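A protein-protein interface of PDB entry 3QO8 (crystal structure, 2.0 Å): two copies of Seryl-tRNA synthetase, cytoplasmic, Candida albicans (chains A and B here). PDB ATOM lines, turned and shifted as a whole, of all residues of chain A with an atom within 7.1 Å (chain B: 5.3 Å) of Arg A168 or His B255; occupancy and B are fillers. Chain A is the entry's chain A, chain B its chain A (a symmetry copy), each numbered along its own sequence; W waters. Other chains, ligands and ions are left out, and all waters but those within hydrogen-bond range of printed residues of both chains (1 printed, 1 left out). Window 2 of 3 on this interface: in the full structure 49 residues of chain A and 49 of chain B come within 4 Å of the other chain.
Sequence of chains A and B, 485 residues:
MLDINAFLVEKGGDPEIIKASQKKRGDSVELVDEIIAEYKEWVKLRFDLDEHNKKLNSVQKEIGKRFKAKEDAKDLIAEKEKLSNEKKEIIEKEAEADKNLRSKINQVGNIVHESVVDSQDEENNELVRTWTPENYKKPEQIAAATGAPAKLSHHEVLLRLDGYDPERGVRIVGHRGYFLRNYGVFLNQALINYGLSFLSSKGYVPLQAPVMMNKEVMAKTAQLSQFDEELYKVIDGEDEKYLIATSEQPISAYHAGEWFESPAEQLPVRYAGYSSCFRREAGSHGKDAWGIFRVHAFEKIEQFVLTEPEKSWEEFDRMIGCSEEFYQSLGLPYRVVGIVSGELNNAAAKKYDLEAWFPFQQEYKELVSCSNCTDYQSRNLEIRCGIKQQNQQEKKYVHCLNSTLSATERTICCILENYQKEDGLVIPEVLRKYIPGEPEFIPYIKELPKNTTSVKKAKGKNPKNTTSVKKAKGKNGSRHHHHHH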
ATOM      1  N   ASP A 162     -10.386  26.962 -32.079  1.00  0.00           N
ATOM      2  CA  ASP A 162      -9.522  26.345 -31.079  1.00  0.00           C
ATOM      3  C   ASP A 162      -9.019  24.997 -31.614  1.00  0.00           C
ATOM      4  O   ASP A 162      -9.068  23.988 -30.915  1.00  0.00           O
ATOM      5  CB  ASP A 162     -10.274  26.138 -29.763  1.00  0.00           C
ATOM      6  CG  ASP A 162      -9.349  25.794 -28.606  1.00  0.00           C
ATOM      7  OD1 ASP A 162      -8.159  26.196 -28.640  1.00  0.00           O
ATOM      8  OD2 ASP A 162      -9.819  25.123 -27.658  1.00  0.00           O
ATOM      9  N   ASP A 165      -2.563  25.130 -31.806  1.00  0.00           N
ATOM     10  CA  ASP A 165      -1.882  25.992 -30.862  1.00  0.00           C
ATOM     11  C   ASP A 165      -0.487  26.334 -31.371  1.00  0.00           C
ATOM     12  O   ASP A 165       0.475  25.600 -31.122  1.00  0.00           O
ATOM     13  CB  ASP A 165      -1.773  25.298 -29.504  1.00  0.00           C
ATOM     14  CG  ASP A 165      -1.569  26.279 -28.370  1.00  0.00           C
ATOM     15  OD1 ASP A 165      -0.836  27.284 -28.565  1.00  0.00           O
ATOM     16  OD2 ASP A 165      -2.153  26.046 -27.290  1.00  0.00           O
ATOM     17  N   PRO A 166      -0.367  27.447 -32.099  1.00  0.00           N
ATOM     18  CA  PRO A 166       0.954  27.839 -32.593  1.00  0.00           C
ATOM     19  C   PRO A 166       1.820  28.453 -31.497  1.00  0.00           C
ATOM     20  O   PRO A 166       3.045  28.384 -31.572  1.00  0.00           O
ATOM     21  CB  PRO A 166       0.635  28.901 -33.659  1.00  0.00           C
ATOM     22  CG  PRO A 166      -0.679  29.502 -33.197  1.00  0.00           C
ATOM     23  CD  PRO A 166      -1.444  28.331 -32.589  1.00  0.00           C
ATOM     24  N   GLU A 167       1.201  29.061 -30.494  1.00  0.00           N
ATOM     25  CA  GLU A 167       2.000  29.728 -29.472  1.00  0.00           C
ATOM     26  C   GLU A 167       2.776  28.712 -28.623  1.00  0.00           C
ATOM     27  O   GLU A 167       3.982  28.844 -28.425  1.00  0.00           O
ATOM     28  CB  GLU A 167       1.134  30.643 -28.596  1.00  0.00           C
ATOM     29  CG  GLU A 167       1.902  31.270 -27.441  1.00  0.00           C
ATOM     30  CD  GLU A 167       1.227  32.518 -26.873  1.00  0.00           C
ATOM     31  OE1 GLU A 167       0.419  33.153 -27.594  1.00  0.00           O
ATOM     32  OE2 GLU A 167       1.516  32.859 -25.702  1.00  0.00           O
ATOM     33  N   ARG A 168       2.085  27.693 -28.126  1.00  0.00           N
ATOM     34  CA  ARG A 168       2.751  26.671 -27.328  1.00  0.00           C
ATOM     35  C   ARG A 168       3.627  25.806 -28.240  1.00  0.00           C
ATOM     36  O   ARG A 168       4.686  25.332 -27.834  1.00  0.00           O
ATOM     37  CB  ARG A 168       1.720  25.838 -26.557  1.00  0.00           C
ATOM     38  CG  ARG A 168       0.880  26.687 -25.595  1.00  0.00           C
ATOM     39  CD  ARG A 168      -0.062  25.830 -24.765  1.00  0.00           C
ATOM     40  NE  ARG A 168      -0.696  26.576 -23.678  1.00  0.00           N
ATOM     41  CZ  ARG A 168      -1.904  27.126 -23.753  1.00  0.00           C
ATOM     42  NH1 ARG A 168      -2.611  27.034 -24.870  1.00  0.00           N
ATOM     43  NH2 ARG A 168      -2.412  27.767 -22.711  1.00  0.00           N
ATOM     44  N   GLY A 169       3.190  25.627 -29.483  1.00  0.00           N
ATOM     45  CA  GLY A 169       4.001  24.954 -30.476  1.00  0.00           C
ATOM     46  C   GLY A 169       5.364  25.613 -30.634  1.00  0.00           C
ATOM     47  O   GLY A 169       6.394  24.950 -30.576  1.00  0.00           O
ATOM     48  N   VAL A 170       5.377  26.928 -30.830  1.00  0.00           N
ATOM     49  CA  VAL A 170       6.642  27.629 -31.028  1.00  0.00           C
ATOM     50  C   VAL A 170       7.553  27.539 -29.809  1.00  0.00           C
ATOM     51  O   VAL A 170       8.749  27.328 -29.949  1.00  0.00           O
ATOM     52  CB  VAL A 170       6.431  29.104 -31.435  1.00  0.00           C
ATOM     53  CG1 VAL A 170       7.739  29.859 -31.370  1.00  0.00           C
ATOM     54  CG2 VAL A 170       5.836  29.177 -32.829  1.00  0.00           C
ATOM     55  N   ARG A 171       6.986  27.674 -28.616  1.00  0.00           N
ATOM     56  CA  ARG A 171       7.784  27.596 -27.396  1.00  0.00           C
ATOM     57  C   ARG A 171       8.472  26.244 -27.244  1.00  0.00           C
ATOM     58  O   ARG A 171       9.596  26.156 -26.754  1.00  0.00           O
ATOM     59  CB  ARG A 171       6.931  27.884 -26.160  1.00  0.00           C
ATOM     60  CG  ARG A 171       7.702  27.731 -24.848  1.00  0.00           C
ATOM     61  CD  ARG A 171       6.927  28.273 -23.655  1.00  0.00           C
ATOM     62  NE  ARG A 171       5.561  27.761 -23.599  1.00  0.00           N
ATOM     63  CZ  ARG A 171       5.241  26.503 -23.304  1.00  0.00           C
ATOM     64  NH1 ARG A 171       6.191  25.607 -23.047  1.00  0.00           N
ATOM     65  NH2 ARG A 171       3.966  26.138 -23.274  1.00  0.00           N
ATOM     66  N   ILE A 172       7.798  25.190 -27.681  1.00  0.00           N
ATOM     67  CA  ILE A 172       8.291  23.834 -27.459  1.00  0.00           C
ATOM     68  C   ILE A 172       9.201  23.302 -28.580  1.00  0.00           C
ATOM     69  O   ILE A 172      10.153  22.580 -28.310  1.00  0.00           O
ATOM     70  CB  ILE A 172       7.102  22.882 -27.163  1.00  0.00           C
ATOM     71  CG1 ILE A 172       6.542  23.212 -25.766  1.00  0.00           C
ATOM     72  CG2 ILE A 172       7.524  21.426 -27.280  1.00  0.00           C
ATOM     73  CD1 ILE A 172       5.199  22.609 -25.458  1.00  0.00           C
ATOM     74  N   VAL A 173       8.924  23.697 -29.823  1.00  0.00           N
ATOM     75  CA  VAL A 173       9.628  23.175 -30.994  1.00  0.00           C
ATOM     76  C   VAL A 173      10.454  24.233 -31.749  1.00  0.00           C
ATOM     77  O   VAL A 173      11.413  23.901 -32.436  1.00  0.00           O
ATOM     78  CB  VAL A 173       8.630  22.611 -32.031  1.00  0.00           C
ATOM     79  CG1 VAL A 173       9.351  21.677 -32.992  1.00  0.00           C
ATOM     80  CG2 VAL A 173       7.487  21.907 -31.343  1.00  0.00           C
ATOM     81  N   GLY A 174      10.063  25.496 -31.638  1.00  0.00           N
ATOM     82  CA  GLY A 174      10.690  26.561 -32.413  1.00  0.00           C
ATOM     83  C   GLY A 174       9.769  26.987 -33.545  1.00  0.00           C
ATOM     84  O   GLY A 174       8.605  26.582 -33.593  1.00  0.00           O
ATOM     85  N   GLY A 177       6.391  25.523 -35.257  1.00  0.00           N
ATOM     86  CA  GLY A 177       5.941  24.412 -34.423  1.00  0.00           C
ATOM     87  C   GLY A 177       4.472  24.531 -34.076  1.00  0.00           C
ATOM     88  O   GLY A 177       3.985  25.633 -33.908  1.00  0.00           O
ATOM     89  N   TYR A 178       3.763  23.407 -33.944  1.00  0.00           N
ATOM     90  CA  TYR A 178       2.342  23.464 -33.603  1.00  0.00           C
ATOM     91  C   TYR A 178       1.852  22.189 -32.946  1.00  0.00           C
ATOM     92  O   TYR A 178       2.403  21.108 -33.178  1.00  0.00           O
ATOM     93  CB  TYR A 178       1.479  23.711 -34.852  1.00  0.00           C
ATOM     94  CG  TYR A 178       1.562  22.595 -35.880  1.00  0.00           C
ATOM     95  CD1 TYR A 178       0.568  21.624 -35.970  1.00  0.00           C
ATOM     96  CD2 TYR A 178       2.638  22.515 -36.759  1.00  0.00           C
ATOM     97  CE1 TYR A 178       0.648  20.600 -36.913  1.00  0.00           C
ATOM     98  CE2 TYR A 178       2.721  21.502 -37.704  1.00  0.00           C
ATOM     99  CZ  TYR A 178       1.727  20.551 -37.777  1.00  0.00           C
ATOM    100  OH  TYR A 178       1.812  19.553 -38.726  1.00  0.00           O
ATOM    101  N   PHE A 179       0.812  22.338 -32.129  1.00  0.00           N
ATOM    102  CA  PHE A 179      -0.019  21.215 -31.704  1.00  0.00           C
ATOM    103  C   PHE A 179      -1.315  21.334 -32.487  1.00  0.00           C
ATOM    104  O   PHE A 179      -1.763  22.447 -32.744  1.00  0.00           O
ATOM    105  CB  PHE A 179      -0.396  21.353 -30.235  1.00  0.00           C
ATOM    106  CG  PHE A 179       0.738  21.139 -29.271  1.00  0.00           C
ATOM    107  CD1 PHE A 179       0.775  19.997 -28.471  1.00  0.00           C
ATOM    108  CD2 PHE A 179       1.741  22.093 -29.127  1.00  0.00           C
ATOM    109  CE1 PHE A 179       1.805  19.796 -27.561  1.00  0.00           C
ATOM    110  CE2 PHE A 179       2.776  21.902 -28.221  1.00  0.00           C
ATOM    111  CZ  PHE A 179       2.812  20.747 -27.432  1.00  0.00           C
ATOM    112  N   ARG A 181      -5.407  20.557 -32.040  1.00  0.00           N
ATOM    113  CA  ARG A 181      -6.294  20.404 -30.877  1.00  0.00           C
ATOM    114  C   ARG A 181      -7.720  20.109 -31.309  1.00  0.00           C
ATOM    115  O   ARG A 181      -8.182  20.649 -32.319  1.00  0.00           O
ATOM    116  CB  ARG A 181      -6.371  21.717 -30.077  1.00  0.00           C
ATOM    117  CG  ARG A 181      -5.174  22.089 -29.261  1.00  0.00           C
ATOM    118  CD  ARG A 181      -5.381  23.483 -28.643  1.00  0.00           C
ATOM    119  NE  ARG A 181      -6.680  23.591 -27.974  1.00  0.00           N
ATOM    120  CZ  ARG A 181      -6.898  23.352 -26.682  1.00  0.00           C
ATOM    121  NH1 ARG A 181      -5.901  22.988 -25.872  1.00  0.00           N
ATOM    122  NH2 ARG A 181      -8.121  23.487 -26.195  1.00  0.00           N
ATOM    123  N   LYS A 446     -13.566  30.860 -30.020  1.00  0.00           N
ATOM    124  CA  LYS A 446     -12.751  31.974 -29.547  1.00  0.00           C
ATOM    125  C   LYS A 446     -12.892  33.134 -30.518  1.00  0.00           C
ATOM    126  O   LYS A 446     -13.213  32.924 -31.684  1.00  0.00           O
ATOM    127  CB  LYS A 446     -11.277  31.556 -29.476  1.00  0.00           C
ATOM    128  CG  LYS A 446     -11.034  30.270 -28.682  1.00  0.00           C
ATOM    129  CD  LYS A 446      -9.560  30.035 -28.365  1.00  0.00           C
ATOM    130  CE  LYS A 446      -8.760  29.752 -29.624  1.00  0.00           C
ATOM    131  NZ  LYS A 446      -7.381  29.245 -29.351  1.00  0.00           N
ATOM    132  N   ILE B 251       3.574  17.312 -24.257  1.00  0.00           N
ATOM    133  CA  ILE B 251       2.319  17.686 -23.626  1.00  0.00           C
ATOM    134  C   ILE B 251       2.547  18.116 -22.171  1.00  0.00           C
ATOM    135  O   ILE B 251       1.858  18.995 -21.659  1.00  0.00           O
ATOM    136  CB  ILE B 251       1.265  16.553 -23.749  1.00  0.00           C
ATOM    137  CG1 ILE B 251       0.934  16.325 -25.232  1.00  0.00           C
ATOM    138  CG2 ILE B 251       0.014  16.894 -22.915  1.00  0.00           C
ATOM    139  CD1 ILE B 251      -0.072  15.187 -25.533  1.00  0.00           C
ATOM    140  N   SER B 252       3.526  17.515 -21.496  1.00  0.00           N
ATOM    141  CA  SER B 252       3.828  17.942 -20.133  1.00  0.00           C
ATOM    142  C   SER B 252       4.311  19.398 -20.144  1.00  0.00           C
ATOM    143  O   SER B 252       4.078  20.145 -19.198  1.00  0.00           O
ATOM    144  CB  SER B 252       4.868  17.029 -19.460  1.00  0.00           C
ATOM    145  OG  SER B 252       6.169  17.244 -19.988  1.00  0.00           O
ATOM    146  N   ALA B 253       4.971  19.804 -21.229  1.00  0.00           N
ATOM    147  CA  ALA B 253       5.478  21.175 -21.327  1.00  0.00           C
ATOM    148  C   ALA B 253       4.445  22.148 -21.898  1.00  0.00           C
ATOM    149  O   ALA B 253       4.703  23.344 -21.974  1.00  0.00           O
ATOM    150  CB  ALA B 253       6.741  21.216 -22.166  1.00  0.00           C
ATOM    151  N   TYR B 254       3.293  21.625 -22.309  1.00  0.00           N
ATOM    152  CA  TYR B 254       2.237  22.429 -22.939  1.00  0.00           C
ATOM    153  C   TYR B 254       1.851  23.634 -22.070  1.00  0.00           C
ATOM    154  O   TYR B 254       1.729  24.753 -22.570  1.00  0.00           O
ATOM    155  CB  TYR B 254       1.016  21.542 -23.202  1.00  0.00           C
ATOM    156  CG  TYR B 254      -0.083  22.130 -24.074  1.00  0.00           C
ATOM    157  CD1 TYR B 254       0.086  22.267 -25.451  1.00  0.00           C
ATOM    158  CD2 TYR B 254      -1.305  22.494 -23.528  1.00  0.00           C
ATOM    159  CE1 TYR B 254      -0.926  22.769 -26.258  1.00  0.00           C
ATOM    160  CE2 TYR B 254      -2.327  23.003 -24.325  1.00  0.00           C
ATOM    161  CZ  TYR B 254      -2.128  23.131 -25.689  1.00  0.00           C
ATOM    162  OH  TYR B 254      -3.132  23.641 -26.473  1.00  0.00           O
ATOM    163  N   HIS B 255       1.661  23.403 -20.774  1.00  0.00           N
ATOM    164  CA  HIS B 255       1.266  24.474 -19.855  1.00  0.00           C
ATOM    165  C   HIS B 255       2.427  25.014 -19.024  1.00  0.00           C
ATOM    166  O   HIS B 255       2.203  25.656 -17.998  1.00  0.00           O
ATOM    167  CB  HIS B 255       0.147  24.006 -18.915  1.00  0.00           C
ATOM    168  CG  HIS B 255      -1.155  23.766 -19.603  1.00  0.00           C
ATOM    169  ND1 HIS B 255      -1.902  24.786 -20.158  1.00  0.00           N
ATOM    170  CD2 HIS B 255      -1.852  22.625 -19.827  1.00  0.00           C
ATOM    171  CE1 HIS B 255      -2.992  24.280 -20.707  1.00  0.00           C
ATOM    172  NE2 HIS B 255      -2.987  22.973 -20.516  1.00  0.00           N
ATOM    173  N   ALA B 256       3.662  24.755 -19.455  1.00  0.00           N
ATOM    174  CA  ALA B 256       4.830  25.300 -18.760  1.00  0.00           C
ATOM    175  C   ALA B 256       4.678  26.807 -18.558  1.00  0.00           C
ATOM    176  O   ALA B 256       4.264  27.528 -19.480  1.00  0.00           O
ATOM    177  CB  ALA B 256       6.108  25.021 -19.548  1.00  0.00           C
ATOM    178  N   GLY B 257       5.019  27.274 -17.357  1.00  0.00           N
ATOM    179  CA  GLY B 257       5.009  28.691 -17.034  1.00  0.00           C
ATOM    180  C   GLY B 257       3.618  29.275 -16.925  1.00  0.00           C
ATOM    181  O   GLY B 257       3.453  30.489 -16.949  1.00  0.00           O
ATOM    182  N   GLU B 258       2.610  28.415 -16.819  1.00  0.00           N
ATOM    183  CA  GLU B 258       1.233  28.880 -16.694  1.00  0.00           C
ATOM    184  C   GLU B 258       0.735  28.648 -15.272  1.00  0.00           C
ATOM    185  O   GLU B 258       1.414  28.021 -14.467  1.00  0.00           O
ATOM    186  CB  GLU B 258       0.323  28.218 -17.740  1.00  0.00           C
ATOM    187  CG  GLU B 258       0.696  28.619 -19.169  1.00  0.00           C
ATOM    188  CD  GLU B 258      -0.116  27.891 -20.234  1.00  0.00           C
ATOM    189  OE1 GLU B 258      -1.255  27.467 -19.951  1.00  0.00           O
ATOM    190  OE2 GLU B 258       0.392  27.749 -21.359  1.00  0.00           O
ATOM    191  N   PHE B 260      -2.790  27.805 -12.994  1.00  0.00           N
ATOM    192  CA  PHE B 260      -4.196  27.501 -12.811  1.00  0.00           C
ATOM    193  C   PHE B 260      -4.629  28.121 -11.486  1.00  0.00           C
ATOM    194  O   PHE B 260      -4.618  27.470 -10.445  1.00  0.00           O
ATOM    195  CB  PHE B 260      -4.427  25.984 -12.856  1.00  0.00           C
ATOM    196  CG  PHE B 260      -4.100  25.372 -14.196  1.00  0.00           C
ATOM    197  CD1 PHE B 260      -5.034  25.379 -15.222  1.00  0.00           C
ATOM    198  CD2 PHE B 260      -2.851  24.820 -14.436  1.00  0.00           C
ATOM    199  CE1 PHE B 260      -4.734  24.822 -16.459  1.00  0.00           C
ATOM    200  CE2 PHE B 260      -2.545  24.265 -15.670  1.00  0.00           C
ATOM    201  CZ  PHE B 260      -3.486  24.265 -16.679  1.00  0.00           C
ATOM    202  N   VAL B 269      -7.470  19.147 -16.022  1.00  0.00           N
ATOM    203  CA  VAL B 269      -7.378  19.265 -17.472  1.00  0.00           C
ATOM    204  C   VAL B 269      -6.882  17.920 -18.006  1.00  0.00           C
ATOM    205  O   VAL B 269      -5.842  17.432 -17.571  1.00  0.00           O
ATOM    206  CB  VAL B 269      -6.398  20.376 -17.875  1.00  0.00           C
ATOM    207  CG1 VAL B 269      -6.018  20.248 -19.323  1.00  0.00           C
ATOM    208  CG2 VAL B 269      -6.991  21.758 -17.580  1.00  0.00           C
ATOM    209  N   TYR B 271      -5.872  15.542 -21.350  1.00  0.00           N
ATOM    210  CA  TYR B 271      -5.529  15.489 -22.774  1.00  0.00           C
ATOM    211  C   TYR B 271      -5.431  14.045 -23.285  1.00  0.00           C
ATOM    212  O   TYR B 271      -4.828  13.186 -22.641  1.00  0.00           O
ATOM    213  CB  TYR B 271      -4.212  16.204 -23.051  1.00  0.00           C
ATOM    214  CG  TYR B 271      -4.294  17.688 -22.799  1.00  0.00           C
ATOM    215  CD1 TYR B 271      -5.107  18.499 -23.590  1.00  0.00           C
ATOM    216  CD2 TYR B 271      -3.590  18.275 -21.763  1.00  0.00           C
ATOM    217  CE1 TYR B 271      -5.207  19.882 -23.350  1.00  0.00           C
ATOM    218  CE2 TYR B 271      -3.680  19.641 -21.521  1.00  0.00           C
ATOM    219  CZ  TYR B 271      -4.486  20.435 -22.321  1.00  0.00           C
ATOM    220  OH  TYR B 271      -4.573  21.788 -22.068  1.00  0.00           O
ATOM    221  N   LEU B 306      -3.599  16.996 -15.659  1.00  0.00           N
ATOM    222  CA  LEU B 306      -3.137  17.884 -14.612  1.00  0.00           C
ATOM    223  C   LEU B 306      -4.288  18.039 -13.639  1.00  0.00           C
ATOM    224  O   LEU B 306      -5.433  18.242 -14.049  1.00  0.00           O
ATOM    225  CB  LEU B 306      -2.762  19.256 -15.199  1.00  0.00           C
ATOM    226  CG  LEU B 306      -1.668  19.341 -16.262  1.00  0.00           C
ATOM    227  CD1 LEU B 306      -2.208  18.928 -17.613  1.00  0.00           C
ATOM    228  CD2 LEU B 306      -1.150  20.785 -16.369  1.00  0.00           C
ATOM    229  N   LEU B 381       8.713  22.751 -14.656  1.00  0.00           N
ATOM    230  CA  LEU B 381       8.081  23.472 -15.763  1.00  0.00           C
ATOM    231  C   LEU B 381       7.307  24.705 -15.289  1.00  0.00           C
ATOM    232  O   LEU B 381       6.740  25.444 -16.098  1.00  0.00           O
ATOM    233  CB  LEU B 381       7.159  22.513 -16.512  1.00  0.00           C
ATOM    234  CG  LEU B 381       7.909  21.406 -17.262  1.00  0.00           C
ATOM    235  CD1 LEU B 381       7.005  20.194 -17.525  1.00  0.00           C
ATOM    236  CD2 LEU B 381       8.494  21.954 -18.567  1.00  0.00           C
ATOM    237  N   GLU B 382       7.294  24.914 -13.975  1.00  0.00           N
ATOM    238  CA  GLU B 382       6.586  26.037 -13.358  1.00  0.00           C
ATOM    239  C   GLU B 382       5.117  26.086 -13.762  1.00  0.00           C
ATOM    240  O   GLU B 382       4.651  27.069 -14.351  1.00  0.00           O
ATOM    241  CB  GLU B 382       7.278  27.368 -13.679  1.00  0.00           C
ATOM    242  CG  GLU B 382       8.717  27.455 -13.188  1.00  0.00           C
ATOM    243  CD  GLU B 382       8.830  27.587 -11.678  1.00  0.00           C
ATOM    244  OE1 GLU B 382       7.794  27.794 -11.011  1.00  0.00           O
ATOM    245  OE2 GLU B 382       9.959  27.493 -11.155  1.00  0.00           O
ATOM    246  N   ILE B 383       4.390  25.021 -13.445  1.00  0.00           N
ATOM    247  CA  ILE B 383       2.958  24.975 -13.698  1.00  0.00           C
ATOM    248  C   ILE B 383       2.225  25.099 -12.368  1.00  0.00           C
ATOM    249  O   ILE B 383       2.033  24.118 -11.650  1.00  0.00           O
ATOM    250  CB  ILE B 383       2.542  23.693 -14.432  1.00  0.00           C
ATOM    251  CG1 ILE B 383       3.416  23.491 -15.669  1.00  0.00           C
ATOM    252  CG2 ILE B 383       1.051  23.750 -14.801  1.00  0.00           C
ATOM    253  CD1 ILE B 383       3.139  22.165 -16.412  1.00  0.00           C
HETATM  254  O   HOH W   1       2.772  28.566 -22.252  1.00  0.00           O
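The side-chain carboxylate (OD2) of Asp A165 lies within hydrogen-bond range of the side-chain hydroxyl (OH) of Tyr B254 (2.7 Å).
The guanidinium group (NE) of Arg A168 sits close to the backbone carbonyl oxygen (O) of Tyr B254, 3.2 Å away.
The side-chain carboxylate of Glu B258 lies within salt-bridge range of the guanidinium group of Arg A168 (2.8 Å).
O of Ala B253 is in hydrogen-bond range of NH1 of Arg A171.
O of Tyr B254 sits at hydrogen-bond distance from NH2 of Arg A171.
The side-chain hydroxyl of Tyr B254 sits at hydrogen-bond distance from the guanidinium group of Arg A181, at 2.9 Å.
NH2 of Arg A181 lies within salt-bridge range of OD2 of Asp A162 (2.8 Å).
OD2 of Asp A165 is in salt-bridge range of NH1 of Arg A168.
The backbone NH (N) of Asp A165 is in hydrogen-bond range of the backbone carbonyl oxygen (O) of Phe A179 (3.0 Å).
OE1 of Glu B258 lies within hydrogen-bond range of ND1 of His B255 (2.8 Å).
NE2 of His B255 lies within hydrogen-bond range of OH of Tyr B271, at 2.5 Å.
The backbone carbonyl oxygen (O) of Glu B382 is in hydrogen-bond range of the backbone NH (N) of Glu B258.
Among the printed residues, merely in contact across the chains: Arg A168 with His B255 (3.96 Å), Arg A171 with Ala B256 (3.5 Å), Ile A172 with Ala B253 (3.6 Å), Ile A172 with Tyr B254 (3.8 Å) and Phe A179 with Tyr B254 (3.7 Å).
Printed residues of chain B within 4 Å of Arg A168: Tyr B254 (3.0 Å), His B255 (3.96 Å) and Glu B258 (2.8 Å).
Printed residues of chain A within 4 Å of His B255: Arg A168 (3.96 Å).
Of the printed residues of chain B, Phe A179 touches Tyr B254.
Printed residues of chain B within 4 Å of Arg A181: Tyr B254.
Ile B383 touches none of the printed residues of chain A.
The nearest printed residue of chain B that does not touch Arg A168 is Ala B253 (6.0 Å).
Of the 15 printed residues of chain B, 5 touch a printed residue of chain A.
Hydrophobic or aromatic side chains of chain B within 4 Å of the printed part of chain A: Ala B253, Tyr B254, His B255 and Ala B256.
Hydrophobic or aromatic side chains of chain A within 4 Å of the printed part of chain B: Ile A172 and Phe A179.
Among the printed residues, 11 pairs touch across the chains.
Among the printed residues, Asp or Glu carboxylates within 4 Å of a Lys or Arg side-chain nitrogen of the other chain: Arg A168 with Glu B258.
No position is printed for both chains.
Water W1 lies within hydrogen-bond range of OE2 of Glu B258 (2.7 Å), NH2 of Arg A171 (2.9 Å) and O of Ala B256 (3.3 Å).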
